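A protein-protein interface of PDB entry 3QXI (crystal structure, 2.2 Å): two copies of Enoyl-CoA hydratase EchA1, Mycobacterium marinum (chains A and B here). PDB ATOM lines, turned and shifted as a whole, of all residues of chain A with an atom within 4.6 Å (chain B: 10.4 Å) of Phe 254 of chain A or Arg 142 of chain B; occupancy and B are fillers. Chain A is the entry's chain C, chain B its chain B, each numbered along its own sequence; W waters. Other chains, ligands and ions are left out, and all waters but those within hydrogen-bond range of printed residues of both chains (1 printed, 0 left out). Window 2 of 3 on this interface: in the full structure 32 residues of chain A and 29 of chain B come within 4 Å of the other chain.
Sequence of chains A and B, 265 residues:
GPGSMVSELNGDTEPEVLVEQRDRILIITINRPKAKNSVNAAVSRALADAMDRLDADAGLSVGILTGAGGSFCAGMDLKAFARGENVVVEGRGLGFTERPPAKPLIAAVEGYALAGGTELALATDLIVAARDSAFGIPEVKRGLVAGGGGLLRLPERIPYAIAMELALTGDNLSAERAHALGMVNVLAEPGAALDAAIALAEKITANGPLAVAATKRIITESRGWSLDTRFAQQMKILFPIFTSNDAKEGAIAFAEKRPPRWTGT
No position is printed for both chains. Of the 8 pairs that touch across the chains among the printed residues, none has its exchanged pair printed and touching as well.
Of the 12 printed residues of chain A, 5 touch a printed residue of chain B. Along chain A the printed residues that touch a printed residue of chain B span positions 246 to 262. Among the printed residues, no Asp or Glu carboxylate lies within 4 Å of a Lys or Arg side-chain nitrogen of the other chain.
Water W1 lies within hydrogen-bond range of O of Ala 247 of chain A (2.7 Å), O of Arg 142 of chain B (3.0 Å) and N of Ala 251 of chain A (3.4 Å).
The backbone carbonyl oxygen (O) of Glu 139 of chain B sits at hydrogen-bond distance from the backbone NH (N) of Leu 144 of chain B, 3.1 Å away. The backbone carbonyl oxygen of Thr 169 of chain B sits at hydrogen-bond distance from the side-chain amino group of Lys 141 of chain B (3.0 Å).
Among the printed residues, pairs that only touch across the chains: Asp 246 of chain A with Arg 142 of chain B (3.9 Å), Ala 247 of chain A with Gly 143 of chain B (3.7 Å), Ala 247 of chain A with Leu 144 of chain B (3.8 Å), Gly 250 of chain A with Arg 142 of chain B (3.4 Å), Phe 254 of chain A with Arg 142 of chain B (3.2 Å), Trp 262 of chain A with Lys 141 of chain B (3.4 Å), Trp 262 of chain A with Arg 142 of chain B (3.6 Å) and Trp 262 of chain A with Gly 143 of chain B (3.5 Å).
Phe 254 of chain A touches just one residue of chain B: Arg 142 (3.2 Å). Of chain A, only Asp 246, Gly 250, Phe 254 and Trp 262 come within 4 Å of Arg 142 of chain B. Ala 247 of chain A touches just these residues of chain B: Gly 143 (3.7 Å) and Leu 144 (3.8 Å). Gly 250 of chain A touches just one residue of chain B: Arg 142. No residue of chain B comes within 4 Å of Ala 251 of chain A. No residue of chain B comes within 4 Å of Ala 253 of chain A. No residue of chain B comes within 4 Å of Ala 255 of chain A. Printed residues of chain A within 4 Å of Gly 143 of chain B: Ala 247 (3.7 Å) and Trp 262 (3.5 Å). Printed residues of chain A within 4 Å of Leu 144 of chain B: Ala 247 (3.8 Å). Of the printed residues of chain B, Trp 262 of chain A touches Lys 141, Arg 142 and Gly 143. Printed residues of chain B within 4 Å of Asp 246 of chain A: Arg 142 (3.9 Å). Printed residues of chain A within 4 Å of Lys 141 of chain B: Trp 262. Asp 77 of chain B touches none of the printed residues of chain A. Ala 146 of chain B touches none of the printed residues of chain A. The nearest residue of chain A that does not touch Arg 142 of chain B is Ala 247 of chain A (4.04 Å). The nearest printed residue of chain B that does not touch Asp 246 of chain A is Gly 143 of chain B (4.5 Å).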
ATOM      1  N   ASP A 246     -20.292   7.425 -14.676  1.00  0.00           N
ATOM      2  CA  ASP A 246     -19.265   8.196 -13.958  1.00  0.00           C
ATOM      3  C   ASP A 246     -18.991   9.544 -14.615  1.00  0.00           C
ATOM      4  O   ASP A 246     -18.851  10.544 -13.926  1.00  0.00           O
ATOM      5  CB  ASP A 246     -17.955   7.400 -13.814  1.00  0.00           C
ATOM      6  CG  ASP A 246     -17.986   6.388 -12.672  1.00  0.00           C
ATOM      7  OD1 ASP A 246     -18.952   6.373 -11.874  1.00  0.00           O
ATOM      8  OD2 ASP A 246     -17.019   5.599 -12.555  1.00  0.00           O
ATOM      9  N   ALA A 247     -18.909   9.594 -15.936  1.00  0.00           N
ATOM     10  CA  ALA A 247     -18.748  10.893 -16.599  1.00  0.00           C
ATOM     11  C   ALA A 247     -19.917  11.832 -16.246  1.00  0.00           C
ATOM     12  O   ALA A 247     -19.698  13.020 -15.970  1.00  0.00           O
ATOM     13  CB  ALA A 247     -18.597  10.736 -18.118  1.00  0.00           C
ATOM     14  N   GLY A 250     -19.593  12.814 -12.522  1.00  0.00           N
ATOM     15  CA  GLY A 250     -18.550  13.831 -12.426  1.00  0.00           C
ATOM     16  C   GLY A 250     -19.082  15.221 -12.725  1.00  0.00           C
ATOM     17  O   GLY A 250     -18.705  16.188 -12.054  1.00  0.00           O
ATOM     18  N   ALA A 251     -19.945  15.331 -13.732  1.00  0.00           N
ATOM     19  CA  ALA A 251     -20.495  16.639 -14.109  1.00  0.00           C
ATOM     20  C   ALA A 251     -21.430  17.148 -13.018  1.00  0.00           C
ATOM     21  O   ALA A 251     -21.296  18.294 -12.583  1.00  0.00           O
ATOM     22  CB  ALA A 251     -21.212  16.594 -15.455  1.00  0.00           C
ATOM     23  N   ILE A 252     -22.327  16.273 -12.557  1.00  0.00           N
ATOM     24  CA  ILE A 252     -23.342  16.610 -11.554  1.00  0.00           C
ATOM     25  C   ILE A 252     -22.715  16.929 -10.195  1.00  0.00           C
ATOM     26  O   ILE A 252     -23.118  17.894  -9.531  1.00  0.00           O
ATOM     27  CB  ILE A 252     -24.430  15.493 -11.409  1.00  0.00           C
ATOM     28  CG1 ILE A 252     -25.129  15.214 -12.751  1.00  0.00           C
ATOM     29  CG2 ILE A 252     -25.489  15.895 -10.386  1.00  0.00           C
ATOM     30  CD1 ILE A 252     -25.902  13.889 -12.786  1.00  0.00           C
ATOM     31  N   ALA A 253     -21.741  16.115  -9.787  1.00  0.00           N
ATOM     32  CA  ALA A 253     -20.956  16.387  -8.577  1.00  0.00           C
ATOM     33  C   ALA A 253     -20.181  17.717  -8.661  1.00  0.00           C
ATOM     34  O   ALA A 253     -20.079  18.435  -7.656  1.00  0.00           O
ATOM     35  CB  ALA A 253     -20.019  15.235  -8.259  1.00  0.00           C
ATOM     36  N   PHE A 254     -19.658  18.054  -9.843  1.00  0.00           N
ATOM     37  CA  PHE A 254     -18.975  19.329 -10.020  1.00  0.00           C
ATOM     38  C   PHE A 254     -19.967  20.490 -10.048  1.00  0.00           C
ATOM     39  O   PHE A 254     -19.691  21.544  -9.493  1.00  0.00           O
ATOM     40  CB  PHE A 254     -18.097  19.337 -11.267  1.00  0.00           C
ATOM     41  CG  PHE A 254     -17.239  20.565 -11.390  1.00  0.00           C
ATOM     42  CD1 PHE A 254     -16.134  20.758 -10.533  1.00  0.00           C
ATOM     43  CD2 PHE A 254     -17.539  21.552 -12.350  1.00  0.00           C
ATOM     44  CE1 PHE A 254     -15.322  21.906 -10.636  1.00  0.00           C
ATOM     45  CE2 PHE A 254     -16.735  22.711 -12.469  1.00  0.00           C
ATOM     46  CZ  PHE A 254     -15.616  22.882 -11.605  1.00  0.00           C
ATOM     47  N   ALA A 255     -21.108  20.286 -10.704  1.00  0.00           N
ATOM     48  CA  ALA A 255     -22.214  21.253 -10.706  1.00  0.00           C
ATOM     49  C   ALA A 255     -22.694  21.574  -9.285  1.00  0.00           C
ATOM     50  O   ALA A 255     -22.847  22.745  -8.931  1.00  0.00           O
ATOM     51  CB  ALA A 255     -23.378  20.735 -11.559  1.00  0.00           C
ATOM     52  N   GLU A 256     -22.913  20.529  -8.482  1.00  0.00           N
ATOM     53  CA  GLU A 256     -23.415  20.656  -7.112  1.00  0.00           C
ATOM     54  C   GLU A 256     -22.306  20.995  -6.091  1.00  0.00           C
ATOM     55  O   GLU A 256     -22.576  21.139  -4.904  1.00  0.00           O
ATOM     56  CB  GLU A 256     -24.183  19.378  -6.705  1.00  0.00           C
ATOM     57  CG  GLU A 256     -25.503  19.129  -7.469  1.00  0.00           C
ATOM     58  CD  GLU A 256     -26.168  17.783  -7.142  1.00  0.00           C
ATOM     59  OE1 GLU A 256     -25.752  17.106  -6.174  1.00  0.00           O
ATOM     60  OE2 GLU A 256     -27.118  17.394  -7.857  1.00  0.00           O
ATOM     61  N   LYS A 257     -21.073  21.157  -6.566  1.00  0.00           N
ATOM     62  CA  LYS A 257     -19.877  21.365  -5.719  1.00  0.00           C
ATOM     63  C   LYS A 257     -19.740  20.395  -4.511  1.00  0.00           C
ATOM     64  O   LYS A 257     -19.554  20.815  -3.357  1.00  0.00           O
ATOM     65  CB  LYS A 257     -19.724  22.835  -5.312  1.00  0.00           C
ATOM     66  N   ARG A 258     -19.800  19.097  -4.811  1.00  0.00           N
ATOM     67  CA  ARG A 258     -19.696  18.024  -3.813  1.00  0.00           C
ATOM     68  C   ARG A 258     -18.870  16.850  -4.367  1.00  0.00           C
ATOM     69  O   ARG A 258     -18.779  16.699  -5.581  1.00  0.00           O
ATOM     70  CB  ARG A 258     -21.092  17.519  -3.427  1.00  0.00           C
ATOM     71  CG  ARG A 258     -21.906  17.083  -4.616  1.00  0.00           C
ATOM     72  CD  ARG A 258     -22.685  15.834  -4.331  1.00  0.00           C
ATOM     73  NE  ARG A 258     -23.498  15.481  -5.496  1.00  0.00           N
ATOM     74  CZ  ARG A 258     -23.325  14.403  -6.260  1.00  0.00           C
ATOM     75  NH1 ARG A 258     -22.369  13.517  -6.005  1.00  0.00           N
ATOM     76  NH2 ARG A 258     -24.136  14.200  -7.284  1.00  0.00           N
ATOM     77  N   TRP A 262     -18.494   7.538  -7.375  1.00  0.00           N
ATOM     78  CA  TRP A 262     -18.229   6.690  -8.540  1.00  0.00           C
ATOM     79  C   TRP A 262     -18.847   5.315  -8.427  1.00  0.00           C
ATOM     80  O   TRP A 262     -18.935   4.773  -7.344  1.00  0.00           O
ATOM     81  CB  TRP A 262     -16.729   6.494  -8.739  1.00  0.00           C
ATOM     82  CG  TRP A 262     -15.897   7.758  -8.776  1.00  0.00           C
ATOM     83  CD1 TRP A 262     -14.818   8.041  -7.983  1.00  0.00           C
ATOM     84  CD2 TRP A 262     -16.052   8.883  -9.658  1.00  0.00           C
ATOM     85  NE1 TRP A 262     -14.308   9.263  -8.298  1.00  0.00           N
ATOM     86  CE2 TRP A 262     -15.037   9.802  -9.330  1.00  0.00           C
ATOM     87  CE3 TRP A 262     -16.955   9.203 -10.680  1.00  0.00           C
ATOM     88  CZ2 TRP A 262     -14.884  11.025  -9.996  1.00  0.00           C
ATOM     89  CZ3 TRP A 262     -16.810  10.431 -11.345  1.00  0.00           C
ATOM     90  CH2 TRP A 262     -15.775  11.324 -10.995  1.00  0.00           C
ATOM     91  N   SER B  38     -11.790  28.322 -23.565  1.00  0.00           N
ATOM     92  CA  SER B  38     -12.176  26.938 -23.846  1.00  0.00           C
ATOM     93  C   SER B  38     -12.527  26.741 -25.317  1.00  0.00           C
ATOM     94  O   SER B  38     -12.992  27.663 -25.982  1.00  0.00           O
ATOM     95  CB  SER B  38     -13.283  26.444 -22.898  1.00  0.00           C
ATOM     96  OG  SER B  38     -14.535  27.086 -23.143  1.00  0.00           O
ATOM     97  N   ALA B  74      -8.319  26.732 -20.837  1.00  0.00           N
ATOM     98  CA  ALA B  74      -8.805  25.846 -19.772  1.00  0.00           C
ATOM     99  C   ALA B  74      -9.271  24.493 -20.316  1.00  0.00           C
ATOM    100  O   ALA B  74      -9.750  23.646 -19.555  1.00  0.00           O
ATOM    101  CB  ALA B  74      -9.955  26.521 -18.990  1.00  0.00           C
ATOM    102  N   GLY B  75      -9.133  24.295 -21.628  1.00  0.00           N
ATOM    103  CA  GLY B  75      -9.451  23.021 -22.267  1.00  0.00           C
ATOM    104  C   GLY B  75     -10.641  23.031 -23.212  1.00  0.00           C
ATOM    105  O   GLY B  75     -11.024  24.075 -23.733  1.00  0.00           O
ATOM    106  N   MET B  76     -11.217  21.859 -23.454  1.00  0.00           N
ATOM    107  CA  MET B  76     -12.388  21.750 -24.309  1.00  0.00           C
ATOM    108  C   MET B  76     -13.615  22.343 -23.602  1.00  0.00           C
ATOM    109  O   MET B  76     -13.805  22.172 -22.391  1.00  0.00           O
ATOM    110  CB  MET B  76     -12.625  20.291 -24.745  1.00  0.00           C
ATOM    111  CG  MET B  76     -13.797  20.095 -25.717  1.00  0.00           C
ATOM    112  SD  MET B  76     -14.005  18.391 -26.314  1.00  0.00           S
ATOM    113  CE  MET B  76     -14.715  17.586 -24.864  1.00  0.00           C
ATOM    114  N   ASP B  77     -14.406  23.094 -24.362  1.00  0.00           N
ATOM    115  CA  ASP B  77     -15.714  23.565 -23.908  1.00  0.00           C
ATOM    116  C   ASP B  77     -16.659  22.356 -23.815  1.00  0.00           C
ATOM    117  O   ASP B  77     -17.225  21.908 -24.828  1.00  0.00           O
ATOM    118  CB  ASP B  77     -16.249  24.581 -24.915  1.00  0.00           C
ATOM    119  CG  ASP B  77     -17.416  25.385 -24.381  1.00  0.00           C
ATOM    120  OD1 ASP B  77     -17.481  26.591 -24.727  1.00  0.00           O
ATOM    121  OD2 ASP B  77     -18.248  24.831 -23.628  1.00  0.00           O
ATOM    122  N   LEU B  78     -16.791  21.802 -22.611  1.00  0.00           N
ATOM    123  CA  LEU B  78     -17.572  20.565 -22.396  1.00  0.00           C
ATOM    124  C   LEU B  78     -19.055  20.768 -22.683  1.00  0.00           C
ATOM    125  O   LEU B  78     -19.714  19.873 -23.233  1.00  0.00           O
ATOM    126  CB  LEU B  78     -17.403  20.046 -20.963  1.00  0.00           C
ATOM    127  CG  LEU B  78     -15.973  19.785 -20.481  1.00  0.00           C
ATOM    128  CD1 LEU B  78     -15.950  19.505 -18.979  1.00  0.00           C
ATOM    129  CD2 LEU B  78     -15.287  18.664 -21.287  1.00  0.00           C
ATOM    130  N   LYS B  79     -19.566  21.945 -22.300  1.00  0.00           N
ATOM    131  CA  LYS B  79     -20.959  22.321 -22.538  1.00  0.00           C
ATOM    132  C   LYS B  79     -21.231  22.271 -24.031  1.00  0.00           C
ATOM    133  O   LYS B  79     -22.183  21.620 -24.464  1.00  0.00           O
ATOM    134  CB  LYS B  79     -21.267  23.700 -21.960  1.00  0.00           C
ATOM    135  N   ALA B  82     -21.144  18.654 -25.102  1.00  0.00           N
ATOM    136  CA  ALA B  82     -22.346  17.948 -24.620  1.00  0.00           C
ATOM    137  C   ALA B  82     -23.585  18.341 -25.417  1.00  0.00           C
ATOM    138  O   ALA B  82     -24.437  17.492 -25.695  1.00  0.00           O
ATOM    139  CB  ALA B  82     -22.583  18.186 -23.139  1.00  0.00           C
ATOM    140  N   LEU B 114      -4.807  23.980 -18.994  1.00  0.00           N
ATOM    141  CA  LEU B 114      -5.317  22.746 -18.407  1.00  0.00           C
ATOM    142  C   LEU B 114      -6.135  21.910 -19.387  1.00  0.00           C
ATOM    143  O   LEU B 114      -6.836  22.458 -20.263  1.00  0.00           O
ATOM    144  CB  LEU B 114      -6.174  23.018 -17.152  1.00  0.00           C
ATOM    145  CG  LEU B 114      -5.483  23.609 -15.927  1.00  0.00           C
ATOM    146  CD1 LEU B 114      -6.512  23.934 -14.851  1.00  0.00           C
ATOM    147  CD2 LEU B 114      -4.360  22.692 -15.402  1.00  0.00           C
ATOM    148  N   ALA B 115      -6.045  20.585 -19.220  1.00  0.00           N
ATOM    149  CA  ALA B 115      -6.892  19.647 -19.964  1.00  0.00           C
ATOM    150  C   ALA B 115      -6.600  19.755 -21.472  1.00  0.00           C
ATOM    151  O   ALA B 115      -5.429  19.700 -21.883  1.00  0.00           O
ATOM    152  CB  ALA B 115      -8.416  19.886 -19.617  1.00  0.00           C
ATOM    153  N   ILE B 137      -3.521  17.499 -16.760  1.00  0.00           N
ATOM    154  CA  ILE B 137      -4.664  16.813 -17.346  1.00  0.00           C
ATOM    155  C   ILE B 137      -5.525  16.275 -16.203  1.00  0.00           C
ATOM    156  O   ILE B 137      -5.414  15.091 -15.823  1.00  0.00           O
ATOM    157  CB  ILE B 137      -4.251  15.726 -18.381  1.00  0.00           C
ATOM    158  CG1 ILE B 137      -3.018  14.922 -17.868  1.00  0.00           C
ATOM    159  CG2 ILE B 137      -3.957  16.393 -19.726  1.00  0.00           C
ATOM    160  CD1 ILE B 137      -2.568  13.770 -18.754  1.00  0.00           C
ATOM    161  N   PRO B 138      -6.390  17.157 -15.642  1.00  0.00           N
ATOM    162  CA  PRO B 138      -7.258  16.768 -14.516  1.00  0.00           C
ATOM    163  C   PRO B 138      -8.467  15.882 -14.895  1.00  0.00           C
ATOM    164  O   PRO B 138      -9.252  15.516 -14.005  1.00  0.00           O
ATOM    165  CB  PRO B 138      -7.748  18.116 -13.956  1.00  0.00           C
ATOM    166  CG  PRO B 138      -7.809  19.029 -15.222  1.00  0.00           C
ATOM    167  CD  PRO B 138      -6.600  18.557 -16.072  1.00  0.00           C
ATOM    168  N   GLU B 139      -8.628  15.542 -16.177  1.00  0.00           N
ATOM    169  CA  GLU B 139      -9.825  14.856 -16.671  1.00  0.00           C
ATOM    170  C   GLU B 139     -10.348  13.763 -15.740  1.00  0.00           C
ATOM    171  O   GLU B 139     -11.531  13.779 -15.414  1.00  0.00           O
ATOM    172  CB  GLU B 139      -9.597  14.278 -18.086  1.00  0.00           C
ATOM    173  CG  GLU B 139      -9.755  15.283 -19.246  1.00  0.00           C
ATOM    174  CD  GLU B 139      -8.496  16.138 -19.477  1.00  0.00           C
ATOM    175  OE1 GLU B 139      -7.570  16.127 -18.632  1.00  0.00           O
ATOM    176  OE2 GLU B 139      -8.432  16.818 -20.516  1.00  0.00           O
ATOM    177  N   VAL B 140      -9.482  12.820 -15.329  1.00  0.00           N
ATOM    178  CA  VAL B 140      -9.917  11.669 -14.532  1.00  0.00           C
ATOM    179  C   VAL B 140     -10.615  12.070 -13.252  1.00  0.00           C
ATOM    180  O   VAL B 140     -11.361  11.279 -12.683  1.00  0.00           O
ATOM    181  CB  VAL B 140      -8.750  10.687 -14.137  1.00  0.00           C
ATOM    182  CG1 VAL B 140      -8.249   9.919 -15.339  1.00  0.00           C
ATOM    183  CG2 VAL B 140      -7.612  11.432 -13.398  1.00  0.00           C
ATOM    184  N   LYS B 141     -10.336  13.275 -12.766  1.00  0.00           N
ATOM    185  CA  LYS B 141     -10.892  13.710 -11.483  1.00  0.00           C
ATOM    186  C   LYS B 141     -12.384  13.888 -11.645  1.00  0.00           C
ATOM    187  O   LYS B 141     -13.107  13.869 -10.647  1.00  0.00           O
ATOM    188  CB  LYS B 141     -10.327  15.066 -11.048  1.00  0.00           C
ATOM    189  CG  LYS B 141      -8.982  15.033 -10.365  1.00  0.00           C
ATOM    190  CD  LYS B 141      -8.263  16.357 -10.615  1.00  0.00           C
ATOM    191  CE  LYS B 141      -7.595  16.908  -9.374  1.00  0.00           C
ATOM    192  NZ  LYS B 141      -6.670  15.936  -8.770  1.00  0.00           N
ATOM    193  N   ARG B 142     -12.812  14.138 -12.886  1.00  0.00           N
ATOM    194  CA  ARG B 142     -14.231  14.260 -13.248  1.00  0.00           C
ATOM    195  C   ARG B 142     -14.804  13.060 -14.003  1.00  0.00           C
ATOM    196  O   ARG B 142     -15.939  13.091 -14.498  1.00  0.00           O
ATOM    197  CB  ARG B 142     -14.470  15.567 -13.972  1.00  0.00           C
ATOM    198  CG  ARG B 142     -14.421  16.682 -12.949  1.00  0.00           C
ATOM    199  CD  ARG B 142     -14.298  18.045 -13.534  1.00  0.00           C
ATOM    200  NE  ARG B 142     -15.564  18.498 -14.086  1.00  0.00           N
ATOM    201  CZ  ARG B 142     -15.741  19.719 -14.575  1.00  0.00           C
ATOM    202  NH1 ARG B 142     -14.732  20.583 -14.556  1.00  0.00           N
ATOM    203  NH2 ARG B 142     -16.923  20.075 -15.076  1.00  0.00           N
ATOM    204  N   GLY B 143     -14.040  11.975 -14.002  1.00  0.00           N
ATOM    205  CA  GLY B 143     -14.448  10.742 -14.643  1.00  0.00           C
ATOM    206  C   GLY B 143     -14.366  10.827 -16.148  1.00  0.00           C
ATOM    207  O   GLY B 143     -15.097  10.112 -16.833  1.00  0.00           O
ATOM    208  N   LEU B 144     -13.481  11.699 -16.644  1.00  0.00           N
ATOM    209  CA  LEU B 144     -13.216  11.886 -18.083  1.00  0.00           C
ATOM    210  C   LEU B 144     -11.838  11.374 -18.450  1.00  0.00           C
ATOM    211  O   LEU B 144     -11.023  11.093 -17.587  1.00  0.00           O
ATOM    212  CB  LEU B 144     -13.299  13.373 -18.451  1.00  0.00           C
ATOM    213  CG  LEU B 144     -14.678  14.009 -18.156  1.00  0.00           C
ATOM    214  CD1 LEU B 144     -14.664  15.493 -18.473  1.00  0.00           C
ATOM    215  CD2 LEU B 144     -15.843  13.272 -18.867  1.00  0.00           C
ATOM    216  N   VAL B 145     -11.560  11.272 -19.743  1.00  0.00           N
ATOM    217  CA  VAL B 145     -10.209  10.891 -20.189  1.00  0.00           C
ATOM    218  C   VAL B 145      -9.729  11.906 -21.213  1.00  0.00           C
ATOM    219  O   VAL B 145     -10.503  12.374 -22.085  1.00  0.00           O
ATOM    220  CB  VAL B 145     -10.168   9.452 -20.698  1.00  0.00           C
ATOM    221  CG1 VAL B 145      -8.771   9.061 -21.194  1.00  0.00           C
ATOM    222  CG2 VAL B 145     -10.580   8.476 -19.577  1.00  0.00           C
ATOM    223  N   ALA B 146      -8.478  12.308 -21.085  1.00  0.00           N
ATOM    224  CA  ALA B 146      -7.950  13.257 -22.027  1.00  0.00           C
ATOM    225  C   ALA B 146      -7.873  12.570 -23.390  1.00  0.00           C
ATOM    226  O   ALA B 146      -7.126  11.599 -23.552  1.00  0.00           O
ATOM    227  CB  ALA B 146      -6.591  13.722 -21.573  1.00  0.00           C
ATOM    228  N   ALA B 167      -1.231  11.901 -15.151  1.00  0.00           N
ATOM    229  CA  ALA B 167      -2.440  11.399 -15.832  1.00  0.00           C
ATOM    230  C   ALA B 167      -3.433  10.704 -14.878  1.00  0.00           C
ATOM    231  O   ALA B 167      -4.649  10.907 -14.963  1.00  0.00           O
ATOM    232  CB  ALA B 167      -2.069  10.476 -16.960  1.00  0.00           C
ATOM    233  N   LEU B 168      -2.905   9.908 -13.971  1.00  0.00           N
ATOM    234  CA  LEU B 168      -3.738   9.144 -13.044  1.00  0.00           C
ATOM    235  C   LEU B 168      -4.241   9.963 -11.828  1.00  0.00           C
ATOM    236  O   LEU B 168      -5.365   9.715 -11.321  1.00  0.00           O
ATOM    237  CB  LEU B 168      -2.981   7.898 -12.577  1.00  0.00           C
ATOM    238  CG  LEU B 168      -2.449   6.896 -13.631  1.00  0.00           C
ATOM    239  CD1 LEU B 168      -1.924   5.699 -12.899  1.00  0.00           C
ATOM    240  CD2 LEU B 168      -3.488   6.443 -14.743  1.00  0.00           C
ATOM    241  N   THR B 169      -3.420  10.911 -11.356  1.00  0.00           N
ATOM    242  CA  THR B 169      -3.808  11.800 -10.247  1.00  0.00           C
ATOM    243  C   THR B 169      -4.620  13.035 -10.736  1.00  0.00           C
ATOM    244  O   THR B 169      -5.540  13.505 -10.051  1.00  0.00           O
ATOM    245  CB  THR B 169      -2.557  12.318  -9.454  1.00  0.00           C
ATOM    246  OG1 THR B 169      -1.775  13.152 -10.308  1.00  0.00           O
ATOM    247  CG2 THR B 169      -1.702  11.169  -8.945  1.00  0.00           C
ATOM    248  N   GLY B 170      -4.255  13.562 -11.906  1.00  0.00           N
ATOM    249  CA  GLY B 170      -4.812  14.833 -12.390  1.00  0.00           C
ATOM    250  C   GLY B 170      -4.146  16.079 -11.776  1.00  0.00           C
ATOM    251  O   GLY B 170      -4.640  17.205 -11.972  1.00  0.00           O
ATOM    252  N   ASP B 171      -3.033  15.905 -11.062  1.00  0.00           N
ATOM    253  CA  ASP B 171      -2.335  17.040 -10.402  1.00  0.00           C
ATOM    254  C   ASP B 171      -1.842  18.025 -11.445  1.00  0.00           C
ATOM    255  O   ASP B 171      -1.472  17.607 -12.544  1.00  0.00           O
ATOM    256  CB  ASP B 171      -1.062  16.580  -9.658  1.00  0.00           C
ATOM    257  CG  ASP B 171      -1.348  15.754  -8.409  1.00  0.00           C
ATOM    258  OD1 ASP B 171      -2.531  15.638  -7.987  1.00  0.00           O
ATOM    259  OD2 ASP B 171      -0.364  15.216  -7.834  1.00  0.00           O
HETATM  260  O   HOH W   1     -17.725  14.856 -16.198  1.00  0.00           O
